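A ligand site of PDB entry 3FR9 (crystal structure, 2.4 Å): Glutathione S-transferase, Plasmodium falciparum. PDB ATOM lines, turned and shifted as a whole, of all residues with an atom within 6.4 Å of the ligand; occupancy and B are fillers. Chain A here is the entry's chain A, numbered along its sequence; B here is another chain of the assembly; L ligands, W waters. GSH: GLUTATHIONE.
Water W1 lies within hydrogen-bond range of an oxygen (O31) of the ligand (2.7 Å), the backbone carbonyl oxygen (O) of Glu 57 (2.7 Å) and the side-chain amino group (NZ) of Lys 49 (2.8 Å).
Water W3 lies within hydrogen-bond range of N of Gln 71, O of Pro 60 and O11 of the ligand.
Water W2 lies within hydrogen-bond range of O31 of the ligand and NZ of Lys 130 of chain B.
Water W6 lies within hydrogen-bond range of the backbone carbonyl oxygen (O) of Cys 101 of chain B (2.7 Å), the side-chain carboxylate (OD2) of Asp 105 of chain B (2.7 Å), a nitrogen (N1) of the ligand (3.3 Å) and the side-chain amide nitrogen (NE2) of Gln 71 (3.3 Å).
A nitrogen (N1) of the ligand is in salt-bridge range of the side-chain carboxylate (OD1) of Asp 105 of chain B (2.7 Å).
The backbone NH of Val 59 is in hydrogen-bond range of an oxygen (O2) of the ligand, 2.8 Å away.
O of Val 59 is in hydrogen-bond range of N2 of the ligand (2.8 Å).
N1 of the ligand sits close to NE2 of Gln 71 (2.9 Å).
O11 of the ligand is in hydrogen-bond range of N of Ser 72 (2.9 Å).
The side-chain hydroxyl (OG) of Ser 72 sits close to an oxygen (O12) of the ligand (3.3 Å).
Residues that only touch the ligand: Phe 10, Lys 15, Phe 45, Glu 57, Gln 58 and Pro 60.
Hydrophobic or aromatic side chains that line the ligand: Phe 10, Phe 45, Val 59 and Pro 60.
Of the 21 residues printed, 10 come within 4 Å of the ligand.
Along chain A the residues within 4 Å of the ligand span positions 10 to 72.
The nearest printed residue that does not touch the ligand is Tyr 9 (4.1 Å).
OE1 of Gln 71 sits close to OD1 of Asp 105 of chain B, at 3.2 Å.
OD1 of Asp 105 of chain B lies close to OE1 of Gln 58 (3.1 Å).
The side-chain amide oxygen of Gln 71 sits at hydrogen-bond distance from the side-chain amide nitrogen of Gln 58 (3.4 Å).
OG of Ser 72 is in hydrogen-bond range of O of Lys 15.
The backbone NH (N) of Lys 15 is in hydrogen-bond range of the side-chain hydroxyl (OH) of Tyr 9 (2.9 Å).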
ATOM      1  N   TYR A   9      11.609  32.969  17.654  1.00  0.00           N
ATOM      2  CA  TYR A   9      11.140  33.852  18.715  1.00  0.00           C
ATOM      3  C   TYR A   9      10.439  35.044  18.089  1.00  0.00           C
ATOM      4  O   TYR A   9      10.423  35.199  16.875  1.00  0.00           O
ATOM      5  CB  TYR A   9      12.306  34.309  19.613  1.00  0.00           C
ATOM      6  CG  TYR A   9      11.872  34.908  20.933  1.00  0.00           C
ATOM      7  CD1 TYR A   9      12.084  36.258  21.210  1.00  0.00           C
ATOM      8  CD2 TYR A   9      11.262  34.122  21.909  1.00  0.00           C
ATOM      9  CE1 TYR A   9      11.692  36.816  22.426  1.00  0.00           C
ATOM     10  CE2 TYR A   9      10.865  34.667  23.121  1.00  0.00           C
ATOM     11  CZ  TYR A   9      11.077  36.008  23.377  1.00  0.00           C
ATOM     12  OH  TYR A   9      10.684  36.547  24.577  1.00  0.00           O
ATOM     13  N   PHE A  10       9.839  35.879  18.938  1.00  0.00           N
ATOM     14  CA  PHE A  10       9.245  37.136  18.507  1.00  0.00           C
ATOM     15  C   PHE A  10      10.345  38.155  18.194  1.00  0.00           C
ATOM     16  O   PHE A  10      11.518  37.920  18.497  1.00  0.00           O
ATOM     17  CB  PHE A  10       8.295  37.666  19.587  1.00  0.00           C
ATOM     18  CG  PHE A  10       7.097  36.800  19.798  1.00  0.00           C
ATOM     19  CD1 PHE A  10       7.073  35.855  20.821  1.00  0.00           C
ATOM     20  CD2 PHE A  10       5.982  36.909  18.966  1.00  0.00           C
ATOM     21  CE1 PHE A  10       5.953  35.040  21.017  1.00  0.00           C
ATOM     22  CE2 PHE A  10       4.863  36.103  19.158  1.00  0.00           C
ATOM     23  CZ  PHE A  10       4.853  35.167  20.182  1.00  0.00           C
ATOM     24  N   LYS A  15      13.176  36.420  26.070  1.00  0.00           N
ATOM     25  CA  LYS A  15      13.586  35.077  26.457  1.00  0.00           C
ATOM     26  C   LYS A  15      14.606  34.435  25.514  1.00  0.00           C
ATOM     27  O   LYS A  15      15.153  33.372  25.825  1.00  0.00           O
ATOM     28  CB  LYS A  15      12.349  34.168  26.610  1.00  0.00           C
ATOM     29  CG  LYS A  15      11.405  34.550  27.757  1.00  0.00           C
ATOM     30  CD  LYS A  15      11.913  34.068  29.112  1.00  0.00           C
ATOM     31  CE  LYS A  15      10.879  34.324  30.201  1.00  0.00           C
ATOM     32  NZ  LYS A  15      11.335  33.849  31.534  1.00  0.00           N
ATOM     33  N   PHE A  45       2.980  33.344  14.650  1.00  0.00           N
ATOM     34  CA  PHE A  45       3.207  32.464  15.810  1.00  0.00           C
ATOM     35  C   PHE A  45       2.174  31.339  15.835  1.00  0.00           C
ATOM     36  O   PHE A  45       2.505  30.195  16.153  1.00  0.00           O
ATOM     37  CB  PHE A  45       3.161  33.282  17.105  1.00  0.00           C
ATOM     38  CG  PHE A  45       3.411  32.469  18.346  1.00  0.00           C
ATOM     39  CD1 PHE A  45       2.459  32.431  19.370  1.00  0.00           C
ATOM     40  CD2 PHE A  45       4.603  31.763  18.519  1.00  0.00           C
ATOM     41  CE1 PHE A  45       2.697  31.693  20.528  1.00  0.00           C
ATOM     42  CE2 PHE A  45       4.836  31.021  19.669  1.00  0.00           C
ATOM     43  CZ  PHE A  45       3.881  30.989  20.680  1.00  0.00           C
ATOM     44  N   LYS A  49       3.169  27.296  15.427  1.00  0.00           N
ATOM     45  CA  LYS A  49       2.751  26.228  16.344  1.00  0.00           C
ATOM     46  C   LYS A  49       2.154  25.015  15.636  1.00  0.00           C
ATOM     47  O   LYS A  49       2.370  23.875  16.079  1.00  0.00           O
ATOM     48  CB  LYS A  49       1.766  26.759  17.395  1.00  0.00           C
ATOM     49  CG  LYS A  49       2.405  27.653  18.457  1.00  0.00           C
ATOM     50  CD  LYS A  49       1.425  28.029  19.554  1.00  0.00           C
ATOM     51  CE  LYS A  49       0.541  29.200  19.148  1.00  0.00           C
ATOM     52  NZ  LYS A  49      -0.401  29.591  20.242  1.00  0.00           N
ATOM     53  N   PHE A  56       5.578  22.855  24.603  1.00  0.00           N
ATOM     54  CA  PHE A  56       4.822  23.717  25.518  1.00  0.00           C
ATOM     55  C   PHE A  56       4.155  24.913  24.836  1.00  0.00           C
ATOM     56  O   PHE A  56       3.637  25.807  25.520  1.00  0.00           O
ATOM     57  CB  PHE A  56       5.701  24.196  26.679  1.00  0.00           C
ATOM     58  CG  PHE A  56       6.424  23.105  27.411  1.00  0.00           C
ATOM     59  CD1 PHE A  56       7.809  23.060  27.436  1.00  0.00           C
ATOM     60  CD2 PHE A  56       5.717  22.097  28.067  1.00  0.00           C
ATOM     61  CE1 PHE A  56       8.488  22.058  28.108  1.00  0.00           C
ATOM     62  CE2 PHE A  56       6.387  21.088  28.748  1.00  0.00           C
ATOM     63  CZ  PHE A  56       7.765  21.064  28.768  1.00  0.00           C
ATOM     64  N   GLU A  57       4.165  24.914  23.509  1.00  0.00           N
ATOM     65  CA  GLU A  57       3.597  26.003  22.691  1.00  0.00           C
ATOM     66  C   GLU A  57       4.157  27.378  23.041  1.00  0.00           C
ATOM     67  O   GLU A  57       3.449  28.384  23.001  1.00  0.00           O
ATOM     68  CB  GLU A  57       2.060  25.993  22.749  1.00  0.00           C
ATOM     69  CG  GLU A  57       1.423  24.732  22.192  1.00  0.00           C
ATOM     70  CD  GLU A  57      -0.098  24.797  22.127  1.00  0.00           C
ATOM     71  OE1 GLU A  57      -0.727  25.238  23.122  1.00  0.00           O
ATOM     72  OE2 GLU A  57      -0.655  24.412  21.088  1.00  0.00           O
ATOM     73  N   GLN A  58       5.447  27.396  23.374  1.00  0.00           N
ATOM     74  CA  GLN A  58       6.153  28.621  23.724  1.00  0.00           C
ATOM     75  C   GLN A  58       7.395  28.792  22.850  1.00  0.00           C
ATOM     76  O   GLN A  58       7.882  27.846  22.240  1.00  0.00           O
ATOM     77  CB  GLN A  58       6.606  28.603  25.185  1.00  0.00           C
ATOM     78  CG  GLN A  58       5.503  28.585  26.213  1.00  0.00           C
ATOM     79  CD  GLN A  58       6.031  28.293  27.604  1.00  0.00           C
ATOM     80  OE1 GLN A  58       5.520  28.819  28.596  1.00  0.00           O
ATOM     81  NE2 GLN A  58       7.048  27.446  27.687  1.00  0.00           N
ATOM     82  N   VAL A  59       7.890  30.023  22.820  1.00  0.00           N
ATOM     83  CA  VAL A  59       9.210  30.328  22.261  1.00  0.00           C
ATOM     84  C   VAL A  59      10.074  30.948  23.387  1.00  0.00           C
ATOM     85  O   VAL A  59       9.523  31.439  24.367  1.00  0.00           O
ATOM     86  CB  VAL A  59       9.133  31.226  20.986  1.00  0.00           C
ATOM     87  CG1 VAL A  59       8.704  30.406  19.777  1.00  0.00           C
ATOM     88  CG2 VAL A  59       8.203  32.407  21.196  1.00  0.00           C
ATOM     89  N   PRO A  60      11.408  30.933  23.247  1.00  0.00           N
ATOM     90  CA  PRO A  60      12.209  30.508  22.089  1.00  0.00           C
ATOM     91  C   PRO A  60      12.131  29.025  21.776  1.00  0.00           C
ATOM     92  O   PRO A  60      11.924  28.194  22.663  1.00  0.00           O
ATOM     93  CB  PRO A  60      13.635  30.886  22.496  1.00  0.00           C
ATOM     94  CG  PRO A  60      13.627  30.847  23.958  1.00  0.00           C
ATOM     95  CD  PRO A  60      12.267  31.348  24.359  1.00  0.00           C
ATOM     96  N   ALA A  70      13.251  23.354  23.335  1.00  0.00           N
ATOM     97  CA  ALA A  70      12.439  24.385  23.974  1.00  0.00           C
ATOM     98  C   ALA A  70      12.976  24.748  25.348  1.00  0.00           C
ATOM     99  O   ALA A  70      13.837  24.063  25.892  1.00  0.00           O
ATOM    100  CB  ALA A  70      10.988  23.934  24.082  1.00  0.00           C
ATOM    101  N   GLN A  71      12.429  25.839  25.899  1.00  0.00           N
ATOM    102  CA  GLN A  71      12.806  26.375  27.223  1.00  0.00           C
ATOM    103  C   GLN A  71      14.162  27.078  27.204  1.00  0.00           C
ATOM    104  O   GLN A  71      15.211  26.431  27.058  1.00  0.00           O
ATOM    105  CB  GLN A  71      12.734  25.299  28.311  1.00  0.00           C
ATOM    106  CG  GLN A  71      11.331  24.740  28.556  1.00  0.00           C
ATOM    107  CD  GLN A  71      10.430  25.691  29.336  1.00  0.00           C
ATOM    108  OE1 GLN A  71       9.224  25.499  29.399  1.00  0.00           O
ATOM    109  NE2 GLN A  71      11.019  26.727  29.922  1.00  0.00           N
ATOM    110  N   SER A  72      14.123  28.405  27.365  1.00  0.00           N
ATOM    111  CA  SER A  72      15.310  29.269  27.366  1.00  0.00           C
ATOM    112  C   SER A  72      16.462  28.712  28.194  1.00  0.00           C
ATOM    113  O   SER A  72      17.557  28.525  27.686  1.00  0.00           O
ATOM    114  CB  SER A  72      14.967  30.652  27.907  1.00  0.00           C
ATOM    115  OG  SER A  72      14.109  31.340  27.032  1.00  0.00           O
ATOM    116  N   GLN A  73      16.176  28.479  29.475  1.00  0.00           N
ATOM    117  CA  GLN A  73      17.187  28.061  30.450  1.00  0.00           C
ATOM    118  C   GLN A  73      17.817  26.741  30.050  1.00  0.00           C
ATOM    119  O   GLN A  73      19.042  26.593  30.096  1.00  0.00           O
ATOM    120  CB  GLN A  73      16.558  27.929  31.837  1.00  0.00           C
ATOM    121  CG  GLN A  73      15.833  29.157  32.349  1.00  0.00           C
ATOM    122  CD  GLN A  73      15.178  28.897  33.692  1.00  0.00           C
ATOM    123  OE1 GLN A  73      15.848  28.579  34.674  1.00  0.00           O
ATOM    124  NE2 GLN A  73      13.853  29.007  33.729  1.00  0.00           N
ATOM    125  N   GLN A 104      17.357  34.905  36.916  1.00  0.00           N
ATOM    126  CA  GLN A 104      15.962  34.647  36.518  1.00  0.00           C
ATOM    127  C   GLN A 104      14.936  35.235  37.485  1.00  0.00           C
ATOM    128  O   GLN A 104      13.879  35.677  37.061  1.00  0.00           O
ATOM    129  CB  GLN A 104      15.712  33.140  36.323  1.00  0.00           C
ATOM    130  CG  GLN A 104      16.572  32.484  35.233  1.00  0.00           C
ATOM    131  CD  GLN A 104      16.529  33.236  33.912  1.00  0.00           C
ATOM    132  OE1 GLN A 104      17.555  33.705  33.418  1.00  0.00           O
ATOM    133  NE2 GLN A 104      15.345  33.347  33.311  1.00  0.00           N
ATOM    134  N   PHE A 116       4.914  44.046  31.396  1.00  0.00           N
ATOM    135  CA  PHE A 116       3.565  43.924  31.937  1.00  0.00           C
ATOM    136  C   PHE A 116       3.356  44.836  33.130  1.00  0.00           C
ATOM    137  O   PHE A 116       2.394  45.595  33.183  1.00  0.00           O
ATOM    138  CB  PHE A 116       3.270  42.459  32.308  1.00  0.00           C
ATOM    139  CG  PHE A 116       3.767  41.469  31.286  1.00  0.00           C
ATOM    140  CD1 PHE A 116       4.906  40.705  31.535  1.00  0.00           C
ATOM    141  CD2 PHE A 116       3.104  41.306  30.075  1.00  0.00           C
ATOM    142  CE1 PHE A 116       5.373  39.789  30.597  1.00  0.00           C
ATOM    143  CE2 PHE A 116       3.558  40.390  29.133  1.00  0.00           C
ATOM    144  CZ  PHE A 116       4.701  39.629  29.390  1.00  0.00           C
ATOM    145  N   CYS B 101      12.012  22.661  33.365  1.00  0.00           N
ATOM    146  CA  CYS B 101      11.681  24.059  33.094  1.00  0.00           C
ATOM    147  C   CYS B 101      10.197  24.253  32.788  1.00  0.00           C
ATOM    148  O   CYS B 101       9.618  25.284  33.126  1.00  0.00           O
ATOM    149  CB  CYS B 101      12.540  24.582  31.946  1.00  0.00           C
ATOM    150  SG  CYS B 101      14.261  24.899  32.369  1.00  0.00           S
ATOM    151  N   GLY B 102       9.595  23.248  32.148  1.00  0.00           N
ATOM    152  CA  GLY B 102       8.154  23.226  31.890  1.00  0.00           C
ATOM    153  C   GLY B 102       7.346  23.077  33.166  1.00  0.00           C
ATOM    154  O   GLY B 102       6.316  23.736  33.345  1.00  0.00           O
ATOM    155  N   ASP B 105       7.157  26.401  34.950  1.00  0.00           N
ATOM    156  CA  ASP B 105       6.172  27.299  34.332  1.00  0.00           C
ATOM    157  C   ASP B 105       4.779  27.116  34.921  1.00  0.00           C
ATOM    158  O   ASP B 105       4.125  28.091  35.286  1.00  0.00           O
ATOM    159  CB  ASP B 105       6.125  27.098  32.813  1.00  0.00           C
ATOM    160  CG  ASP B 105       7.230  27.824  32.078  1.00  0.00           C
ATOM    161  OD1 ASP B 105       7.320  27.669  30.840  1.00  0.00           O
ATOM    162  OD2 ASP B 105       8.027  28.550  32.717  1.00  0.00           O
ATOM    163  N   LYS B 130      -4.151  22.362  29.972  1.00  0.00           N
ATOM    164  CA  LYS B 130      -3.278  22.608  28.827  1.00  0.00           C
ATOM    165  C   LYS B 130      -1.871  22.068  29.080  1.00  0.00           C
ATOM    166  O   LYS B 130      -1.276  21.431  28.205  1.00  0.00           O
ATOM    167  CB  LYS B 130      -3.236  24.112  28.522  1.00  0.00           C
ATOM    168  CG  LYS B 130      -2.340  24.515  27.364  1.00  0.00           C
ATOM    169  CD  LYS B 130      -2.473  25.990  27.024  1.00  0.00           C
ATOM    170  CE  LYS B 130      -1.731  26.865  28.023  1.00  0.00           C
ATOM    171  NZ  LYS B 130      -1.839  28.304  27.658  1.00  0.00           N
ATOM    172  N   TRP B 131      -1.347  22.318  30.275  1.00  0.00           N
ATOM    173  CA  TRP B 131      -0.023  21.837  30.661  1.00  0.00           C
ATOM    174  C   TRP B 131       0.009  20.338  30.947  1.00  0.00           C
ATOM    175  O   TRP B 131       0.996  19.665  30.653  1.00  0.00           O
ATOM    176  CB  TRP B 131       0.542  22.651  31.820  1.00  0.00           C
ATOM    177  CG  TRP B 131       1.083  23.953  31.350  1.00  0.00           C
ATOM    178  CD1 TRP B 131       0.381  25.103  31.141  1.00  0.00           C
ATOM    179  CD2 TRP B 131       2.432  24.230  30.979  1.00  0.00           C
ATOM    180  NE1 TRP B 131       1.211  26.086  30.679  1.00  0.00           N
ATOM    181  CE2 TRP B 131       2.482  25.585  30.570  1.00  0.00           C
ATOM    182  CE3 TRP B 131       3.614  23.470  30.960  1.00  0.00           C
ATOM    183  CZ2 TRP B 131       3.674  26.189  30.149  1.00  0.00           C
ATOM    184  CZ3 TRP B 131       4.788  24.080  30.546  1.00  0.00           C
ATOM    185  CH2 TRP B 131       4.802  25.428  30.136  1.00  0.00           C
HETATM  186  N1  GSH L   1       9.503  29.157  30.268  1.00  0.00           N
HETATM  187  CA1 GSH L   1       9.885  30.228  29.371  1.00  0.00           C
HETATM  188  C1  GSH L   1      11.254  29.949  28.805  1.00  0.00           C
HETATM  189  O11 GSH L   1      11.415  29.437  27.677  1.00  0.00           O
HETATM  190  O12 GSH L   1      12.260  30.246  29.480  1.00  0.00           O
HETATM  191  CB1 GSH L   1       8.840  30.385  28.275  1.00  0.00           C
HETATM  192  CG1 GSH L   1       8.965  31.758  27.635  1.00  0.00           C
HETATM  193  CD1 GSH L   1       7.616  32.299  27.252  1.00  0.00           C
HETATM  194  OE1 GSH L   1       6.636  32.571  28.243  1.00  0.00           O
HETATM  195  N2  GSH L   1       7.426  32.491  25.951  1.00  0.00           N
HETATM  196  CA2 GSH L   1       6.426  33.399  25.447  1.00  0.00           C
HETATM  197  C2  GSH L   1       5.481  32.664  24.556  1.00  0.00           C
HETATM  198  O2  GSH L   1       5.962  31.998  23.417  1.00  0.00           O
HETATM  199  CB2 GSH L   1       7.087  34.544  24.690  1.00  0.00           C
HETATM  200  SG2 GSH L   1       5.925  35.908  24.367  1.00  0.00           S
HETATM  201  N3  GSH L   1       4.204  32.670  24.910  1.00  0.00           N
HETATM  202  CA3 GSH L   1       3.214  31.860  24.231  1.00  0.00           C
HETATM  203  C3  GSH L   1       1.813  32.116  24.715  1.00  0.00           C
HETATM  204  O31 GSH L   1       0.882  31.353  24.396  1.00  0.00           O
HETATM  205  O32 GSH L   1       1.561  33.108  25.440  1.00  0.00           O
HETATM  206  O   HOH W   1       0.915  29.286  22.660  1.00  0.00           O
HETATM  207  O   HOH W   2      -1.218  31.449  26.620  1.00  0.00           O
HETATM  208  O   HOH W   3      10.591  27.978  25.231  1.00  0.00           O
HETATM  209  O   HOH W   4      13.538  27.836  30.496  1.00  0.00           O
HETATM  210  O   HOH W   5       3.900  33.457  28.131  1.00  0.00           O
HETATM  211  O   HOH W   6      10.624  27.798  33.012  1.00  0.00           O
HETATM  212  O   HOH W   7      13.042  31.249  32.345  1.00  0.00           O
